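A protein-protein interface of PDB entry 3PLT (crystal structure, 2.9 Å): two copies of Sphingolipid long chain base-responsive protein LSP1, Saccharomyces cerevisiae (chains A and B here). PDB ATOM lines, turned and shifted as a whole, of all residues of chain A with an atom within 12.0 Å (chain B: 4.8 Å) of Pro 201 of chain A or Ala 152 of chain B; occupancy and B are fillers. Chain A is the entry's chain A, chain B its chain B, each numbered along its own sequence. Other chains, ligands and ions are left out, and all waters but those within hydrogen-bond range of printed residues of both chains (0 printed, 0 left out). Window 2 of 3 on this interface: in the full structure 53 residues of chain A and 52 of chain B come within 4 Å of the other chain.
No position is printed for both chains.
Printed residues of chain A that touch a printed residue of chain B: Asp 61, Pro 198, Val 199, Pro 201 and Gly 202.
Of the 10 printed residues of chain B, 4 touch a printed residue of chain A.
Along chain B the printed residues that touch a printed residue of chain A span positions 148 to 156.
Among the printed residues, 5 pairs touch across the chains.
The side-chain amide oxygen of Asn 156 of chain B sits at hydrogen-bond distance from the backbone NH of Val 199 of chain A.
Among the printed residues, merely in contact across the chains: Pro 198 of chain A with Asn 156 of chain B (3.3 Å), Gly 202 of chain A with Leu 148 of chain B (3.6 Å), Pro 201 of chain A with Ala 152 of chain B (3.7 Å) and Asp 61 of chain A with Ser 155 of chain B (3.7 Å).
Of the printed residues of chain B, Pro 201 of chain A touches Ala 152.
Ala 152 of chain B touches just one residue of chain A: Pro 201.
No residue of chain A comes within 4 Å of Val 149 of chain B.
No residue of chain A comes within 4 Å of Ala 150 of chain B.
No residue of chain A comes within 4 Å of Glu 151 of chain B.
Gln 153 of chain B touches none of the printed residues of chain A.
Of the printed residues of chain A, Ser 155 of chain B touches Asp 61.
Asn 156 of chain B touches just these residues of chain A: Pro 198 (3.3 Å) and Val 199 (2.7 Å).
Printed residues of chain B within 4 Å of Gly 202 of chain A: Leu 148.
Printed residues of chain B within 4 Å of Val 199 of chain A: Asn 156 (2.7 Å).
Printed residues of chain B within 4 Å of Asp 61 of chain A: Ser 155 (3.7 Å).
The nearest residue of chain A that does not touch Ala 152 of chain B is Val 199 of chain A (4.5 Å).
The backbone carbonyl oxygen (O) of Ala 152 of chain B sits at hydrogen-bond distance from the side-chain amide nitrogen (ND2) of Asn 156 of chain B, 2.7 Å away.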
ATOM      1  N   ASN A  60       9.262 -30.584  33.747  1.00  0.00           N
ATOM      2  CA  ASN A  60      10.385 -30.003  33.040  1.00  0.00           C
ATOM      3  C   ASN A  60      11.209 -29.162  34.001  1.00  0.00           C
ATOM      4  O   ASN A  60      11.208 -29.423  35.195  1.00  0.00           O
ATOM      5  CB  ASN A  60       9.855 -29.165  31.880  1.00  0.00           C
ATOM      6  CG  ASN A  60      10.610 -29.412  30.590  1.00  0.00           C
ATOM      7  OD1 ASN A  60      11.649 -28.797  30.317  1.00  0.00           O
ATOM      8  ND2 ASN A  60      10.073 -30.309  29.779  1.00  0.00           N
ATOM      9  N   ASP A  61      11.926 -28.171  33.488  1.00  0.00           N
ATOM     10  CA  ASP A  61      12.573 -27.197  34.347  1.00  0.00           C
ATOM     11  C   ASP A  61      11.526 -26.354  35.089  1.00  0.00           C
ATOM     12  O   ASP A  61      10.373 -26.247  34.669  1.00  0.00           O
ATOM     13  CB  ASP A  61      13.528 -26.305  33.540  1.00  0.00           C
ATOM     14  CG  ASP A  61      14.794 -27.048  33.080  1.00  0.00           C
ATOM     15  OD1 ASP A  61      15.049 -28.173  33.575  1.00  0.00           O
ATOM     16  OD2 ASP A  61      15.547 -26.505  32.229  1.00  0.00           O
ATOM     17  N   VAL A  64       9.921 -23.465  32.955  1.00  0.00           N
ATOM     18  CA  VAL A  64       9.022 -23.981  31.940  1.00  0.00           C
ATOM     19  C   VAL A  64       7.746 -24.511  32.588  1.00  0.00           C
ATOM     20  O   VAL A  64       6.651 -24.222  32.116  1.00  0.00           O
ATOM     21  CB  VAL A  64       9.692 -25.088  31.113  1.00  0.00           C
ATOM     22  CG1 VAL A  64       8.670 -25.863  30.319  1.00  0.00           C
ATOM     23  CG2 VAL A  64      10.737 -24.499  30.186  1.00  0.00           C
ATOM     24  N   ASP A 195      13.207 -17.560  30.103  1.00  0.00           N
ATOM     25  CA  ASP A 195      14.526 -17.199  29.582  1.00  0.00           C
ATOM     26  C   ASP A 195      15.007 -18.240  28.583  1.00  0.00           C
ATOM     27  O   ASP A 195      15.107 -19.419  28.924  1.00  0.00           O
ATOM     28  CB  ASP A 195      15.540 -17.111  30.727  1.00  0.00           C
ATOM     29  CG  ASP A 195      16.979 -16.925  30.234  1.00  0.00           C
ATOM     30  OD1 ASP A 195      17.164 -16.438  29.089  1.00  0.00           O
ATOM     31  OD2 ASP A 195      17.923 -17.266  30.991  1.00  0.00           O
ATOM     32  N   ASP A 196      15.342 -17.797  27.371  1.00  0.00           N
ATOM     33  CA  ASP A 196      15.840 -18.702  26.315  1.00  0.00           C
ATOM     34  C   ASP A 196      17.349 -18.613  26.055  1.00  0.00           C
ATOM     35  O   ASP A 196      17.838 -19.117  25.043  1.00  0.00           O
ATOM     36  CB  ASP A 196      15.064 -18.500  25.006  1.00  0.00           C
ATOM     37  CG  ASP A 196      15.275 -17.128  24.386  1.00  0.00           C
ATOM     38  OD1 ASP A 196      15.218 -16.123  25.127  1.00  0.00           O
ATOM     39  OD2 ASP A 196      15.462 -17.067  23.143  1.00  0.00           O
ATOM     40  N   SER A 197      18.078 -17.991  26.982  1.00  0.00           N
ATOM     41  CA  SER A 197      19.535 -17.873  26.897  1.00  0.00           C
ATOM     42  C   SER A 197      20.191 -19.242  26.991  1.00  0.00           C
ATOM     43  O   SER A 197      20.070 -19.911  28.025  1.00  0.00           O
ATOM     44  CB  SER A 197      20.068 -16.986  28.020  1.00  0.00           C
ATOM     45  OG  SER A 197      19.551 -15.683  27.878  1.00  0.00           O
ATOM     46  N   PRO A 198      20.897 -19.656  25.924  1.00  0.00           N
ATOM     47  CA  PRO A 198      21.594 -20.931  25.875  1.00  0.00           C
ATOM     48  C   PRO A 198      22.411 -21.303  27.108  1.00  0.00           C
ATOM     49  O   PRO A 198      22.740 -20.457  27.951  1.00  0.00           O
ATOM     50  CB  PRO A 198      22.531 -20.753  24.688  1.00  0.00           C
ATOM     51  CG  PRO A 198      21.776 -19.903  23.772  1.00  0.00           C
ATOM     52  CD  PRO A 198      21.043 -18.927  24.652  1.00  0.00           C
ATOM     53  N   VAL A 199      22.745 -22.584  27.166  1.00  0.00           N
ATOM     54  CA  VAL A 199      23.471 -23.167  28.267  1.00  0.00           C
ATOM     55  C   VAL A 199      24.710 -23.863  27.723  1.00  0.00           C
ATOM     56  O   VAL A 199      24.698 -24.425  26.623  1.00  0.00           O
ATOM     57  CB  VAL A 199      22.574 -24.160  29.068  1.00  0.00           C
ATOM     58  CG1 VAL A 199      23.307 -25.464  29.379  1.00  0.00           C
ATOM     59  CG2 VAL A 199      22.055 -23.501  30.353  1.00  0.00           C
ATOM     60  N   THR A 200      25.788 -23.783  28.498  1.00  0.00           N
ATOM     61  CA  THR A 200      26.992 -24.546  28.241  1.00  0.00           C
ATOM     62  C   THR A 200      26.741 -25.964  28.733  1.00  0.00           C
ATOM     63  O   THR A 200      26.288 -26.153  29.870  1.00  0.00           O
ATOM     64  CB  THR A 200      28.193 -23.975  29.021  1.00  0.00           C
ATOM     65  OG1 THR A 200      28.338 -22.580  28.732  1.00  0.00           O
ATOM     66  CG2 THR A 200      29.487 -24.709  28.664  1.00  0.00           C
ATOM     67  N   PRO A 201      27.026 -26.965  27.886  1.00  0.00           N
ATOM     68  CA  PRO A 201      27.010 -28.358  28.308  1.00  0.00           C
ATOM     69  C   PRO A 201      27.830 -28.562  29.574  1.00  0.00           C
ATOM     70  O   PRO A 201      29.035 -28.323  29.563  1.00  0.00           O
ATOM     71  CB  PRO A 201      27.666 -29.085  27.132  1.00  0.00           C
ATOM     72  CG  PRO A 201      27.349 -28.246  25.952  1.00  0.00           C
ATOM     73  CD  PRO A 201      27.305 -26.827  26.447  1.00  0.00           C
ATOM     74  N   GLY A 202      27.172 -28.976  30.654  1.00  0.00           N
ATOM     75  CA  GLY A 202      27.821 -29.135  31.953  1.00  0.00           C
ATOM     76  C   GLY A 202      27.150 -28.336  33.055  1.00  0.00           C
ATOM     77  O   GLY A 202      26.567 -28.903  33.977  1.00  0.00           O
ATOM     78  N   GLU A 203      27.225 -27.015  32.970  1.00  0.00           N
ATOM     79  CA  GLU A 203      26.762 -26.191  34.072  1.00  0.00           C
ATOM     80  C   GLU A 203      25.228 -26.085  34.082  1.00  0.00           C
ATOM     81  O   GLU A 203      24.568 -26.366  33.075  1.00  0.00           O
ATOM     82  CB  GLU A 203      27.434 -24.814  34.048  1.00  0.00           C
ATOM     83  CG  GLU A 203      27.384 -24.073  35.395  1.00  0.00           C
ATOM     84  CD  GLU A 203      28.426 -22.973  35.512  1.00  0.00           C
ATOM     85  OE1 GLU A 203      28.058 -21.779  35.368  1.00  0.00           O
ATOM     86  OE2 GLU A 203      29.610 -23.303  35.744  1.00  0.00           O
ATOM     87  N   ALA A 204      24.690 -25.692  35.240  1.00  0.00           N
ATOM     88  CA  ALA A 204      23.263 -25.739  35.536  1.00  0.00           C
ATOM     89  C   ALA A 204      22.543 -24.459  35.147  1.00  0.00           C
ATOM     90  O   ALA A 204      23.173 -23.438  34.891  1.00  0.00           O
ATOM     91  CB  ALA A 204      23.063 -26.008  37.026  1.00  0.00           C
ATOM     92  N   ARG A 205      21.213 -24.534  35.116  1.00  0.00           N
ATOM     93  CA  ARG A 205      20.352 -23.372  34.865  1.00  0.00           C
ATOM     94  C   ARG A 205      20.245 -22.532  36.139  1.00  0.00           C
ATOM     95  O   ARG A 205      20.257 -23.084  37.242  1.00  0.00           O
ATOM     96  CB  ARG A 205      18.942 -23.817  34.439  1.00  0.00           C
ATOM     97  CG  ARG A 205      18.840 -24.377  33.020  1.00  0.00           C
ATOM     98  CD  ARG A 205      18.686 -23.274  32.009  1.00  0.00           C
ATOM     99  NE  ARG A 205      17.303 -22.814  31.932  1.00  0.00           N
ATOM    100  CZ  ARG A 205      16.922 -21.537  31.836  1.00  0.00           C
ATOM    101  NH1 ARG A 205      17.819 -20.546  31.829  1.00  0.00           N
ATOM    102  NH2 ARG A 205      15.625 -21.246  31.758  1.00  0.00           N
ATOM    103  N   PRO A 206      20.123 -21.196  35.997  1.00  0.00           N
ATOM    104  CA  PRO A 206      20.043 -20.311  37.163  1.00  0.00           C
ATOM    105  C   PRO A 206      18.780 -20.451  38.009  1.00  0.00           C
ATOM    106  O   PRO A 206      17.890 -21.238  37.699  1.00  0.00           O
ATOM    107  CB  PRO A 206      20.067 -18.899  36.552  1.00  0.00           C
ATOM    108  CG  PRO A 206      20.510 -19.050  35.167  1.00  0.00           C
ATOM    109  CD  PRO A 206      20.148 -20.434  34.734  1.00  0.00           C
ATOM    110  N   SER B 147      25.835 -37.492  26.764  1.00  0.00           N
ATOM    111  CA  SER B 147      24.659 -37.134  27.564  1.00  0.00           C
ATOM    112  C   SER B 147      24.635 -35.629  27.867  1.00  0.00           C
ATOM    113  O   SER B 147      23.634 -34.948  27.623  1.00  0.00           O
ATOM    114  CB  SER B 147      24.634 -37.962  28.861  1.00  0.00           C
ATOM    115  OG  SER B 147      23.809 -37.386  29.854  1.00  0.00           O
ATOM    116  N   LEU B 148      25.745 -35.121  28.388  1.00  0.00           N
ATOM    117  CA  LEU B 148      25.889 -33.694  28.633  1.00  0.00           C
ATOM    118  C   LEU B 148      25.573 -32.850  27.399  1.00  0.00           C
ATOM    119  O   LEU B 148      24.820 -31.894  27.482  1.00  0.00           O
ATOM    120  CB  LEU B 148      27.308 -33.370  29.117  1.00  0.00           C
ATOM    121  CG  LEU B 148      27.568 -33.503  30.611  1.00  0.00           C
ATOM    122  CD1 LEU B 148      29.041 -33.262  30.888  1.00  0.00           C
ATOM    123  CD2 LEU B 148      26.682 -32.518  31.386  1.00  0.00           C
ATOM    124  N   VAL B 149      26.152 -33.192  26.258  1.00  0.00           N
ATOM    125  CA  VAL B 149      25.921 -32.406  25.060  1.00  0.00           C
ATOM    126  C   VAL B 149      24.475 -32.537  24.631  1.00  0.00           C
ATOM    127  O   VAL B 149      23.860 -31.566  24.204  1.00  0.00           O
ATOM    128  CB  VAL B 149      26.834 -32.836  23.914  1.00  0.00           C
ATOM    129  CG1 VAL B 149      26.401 -32.186  22.609  1.00  0.00           C
ATOM    130  CG2 VAL B 149      28.279 -32.482  24.243  1.00  0.00           C
ATOM    131  N   ALA B 150      23.934 -33.741  24.760  1.00  0.00           N
ATOM    132  CA  ALA B 150      22.539 -34.006  24.424  1.00  0.00           C
ATOM    133  C   ALA B 150      21.578 -33.225  25.323  1.00  0.00           C
ATOM    134  O   ALA B 150      20.667 -32.559  24.836  1.00  0.00           O
ATOM    135  CB  ALA B 150      22.247 -35.506  24.506  1.00  0.00           C
ATOM    136  N   GLU B 151      21.780 -33.291  26.630  1.00  0.00           N
ATOM    137  CA  GLU B 151      20.880 -32.592  27.533  1.00  0.00           C
ATOM    138  C   GLU B 151      20.934 -31.088  27.284  1.00  0.00           C
ATOM    139  O   GLU B 151      19.912 -30.414  27.332  1.00  0.00           O
ATOM    140  CB  GLU B 151      21.207 -32.891  28.995  1.00  0.00           C
ATOM    141  CG  GLU B 151      21.082 -34.362  29.390  1.00  0.00           C
ATOM    142  CD  GLU B 151      19.692 -34.939  29.171  1.00  0.00           C
ATOM    143  OE1 GLU B 151      18.704 -34.186  29.288  1.00  0.00           O
ATOM    144  OE2 GLU B 151      19.593 -36.160  28.882  1.00  0.00           O
ATOM    145  N   ALA B 152      22.130 -30.575  27.014  1.00  0.00           N
ATOM    146  CA  ALA B 152      22.332 -29.155  26.763  1.00  0.00           C
ATOM    147  C   ALA B 152      21.537 -28.713  25.557  1.00  0.00           C
ATOM    148  O   ALA B 152      20.929 -27.655  25.558  1.00  0.00           O
ATOM    149  CB  ALA B 152      23.798 -28.869  26.534  1.00  0.00           C
ATOM    150  N   GLN B 153      21.555 -29.531  24.519  1.00  0.00           N
ATOM    151  CA  GLN B 153      20.872 -29.193  23.286  1.00  0.00           C
ATOM    152  C   GLN B 153      19.348 -29.295  23.478  1.00  0.00           C
ATOM    153  O   GLN B 153      18.597 -28.455  22.980  1.00  0.00           O
ATOM    154  CB  GLN B 153      21.376 -30.102  22.164  1.00  0.00           C
ATOM    155  CG  GLN B 153      20.999 -29.678  20.751  1.00  0.00           C
ATOM    156  CD  GLN B 153      21.308 -30.781  19.711  1.00  0.00           C
ATOM    157  OE1 GLN B 153      22.218 -31.604  19.912  1.00  0.00           O
ATOM    158  NE2 GLN B 153      20.547 -30.794  18.602  1.00  0.00           N
ATOM    159  N   LEU B 154      18.895 -30.302  24.225  1.00  0.00           N
ATOM    160  CA  LEU B 154      17.466 -30.450  24.518  1.00  0.00           C
ATOM    161  C   LEU B 154      16.943 -29.231  25.254  1.00  0.00           C
ATOM    162  O   LEU B 154      15.954 -28.644  24.858  1.00  0.00           O
ATOM    163  CB  LEU B 154      17.201 -31.696  25.364  1.00  0.00           C
ATOM    164  CG  LEU B 154      15.760 -31.846  25.857  1.00  0.00           C
ATOM    165  CD1 LEU B 154      14.821 -31.982  24.662  1.00  0.00           C
ATOM    166  CD2 LEU B 154      15.603 -33.016  26.818  1.00  0.00           C
ATOM    167  N   SER B 155      17.613 -28.864  26.331  1.00  0.00           N
ATOM    168  CA  SER B 155      17.216 -27.726  27.132  1.00  0.00           C
ATOM    169  C   SER B 155      17.147 -26.488  26.257  1.00  0.00           C
ATOM    170  O   SER B 155      16.105 -25.852  26.168  1.00  0.00           O
ATOM    171  CB  SER B 155      18.216 -27.518  28.272  1.00  0.00           C
ATOM    172  OG  SER B 155      17.742 -26.601  29.232  1.00  0.00           O
ATOM    173  N   ASN B 156      18.254 -26.177  25.589  1.00  0.00           N
ATOM    174  CA  ASN B 156      18.396 -24.930  24.826  1.00  0.00           C
ATOM    175  C   ASN B 156      17.414 -24.795  23.674  1.00  0.00           C
ATOM    176  O   ASN B 156      16.965 -23.690  23.373  1.00  0.00           O
ATOM    177  CB  ASN B 156      19.812 -24.800  24.265  1.00  0.00           C
ATOM    178  CG  ASN B 156      20.857 -24.647  25.341  1.00  0.00           C
ATOM    179  OD1 ASN B 156      20.626 -24.018  26.373  1.00  0.00           O
ATOM    180  ND2 ASN B 156      22.025 -25.217  25.103  1.00  0.00           N
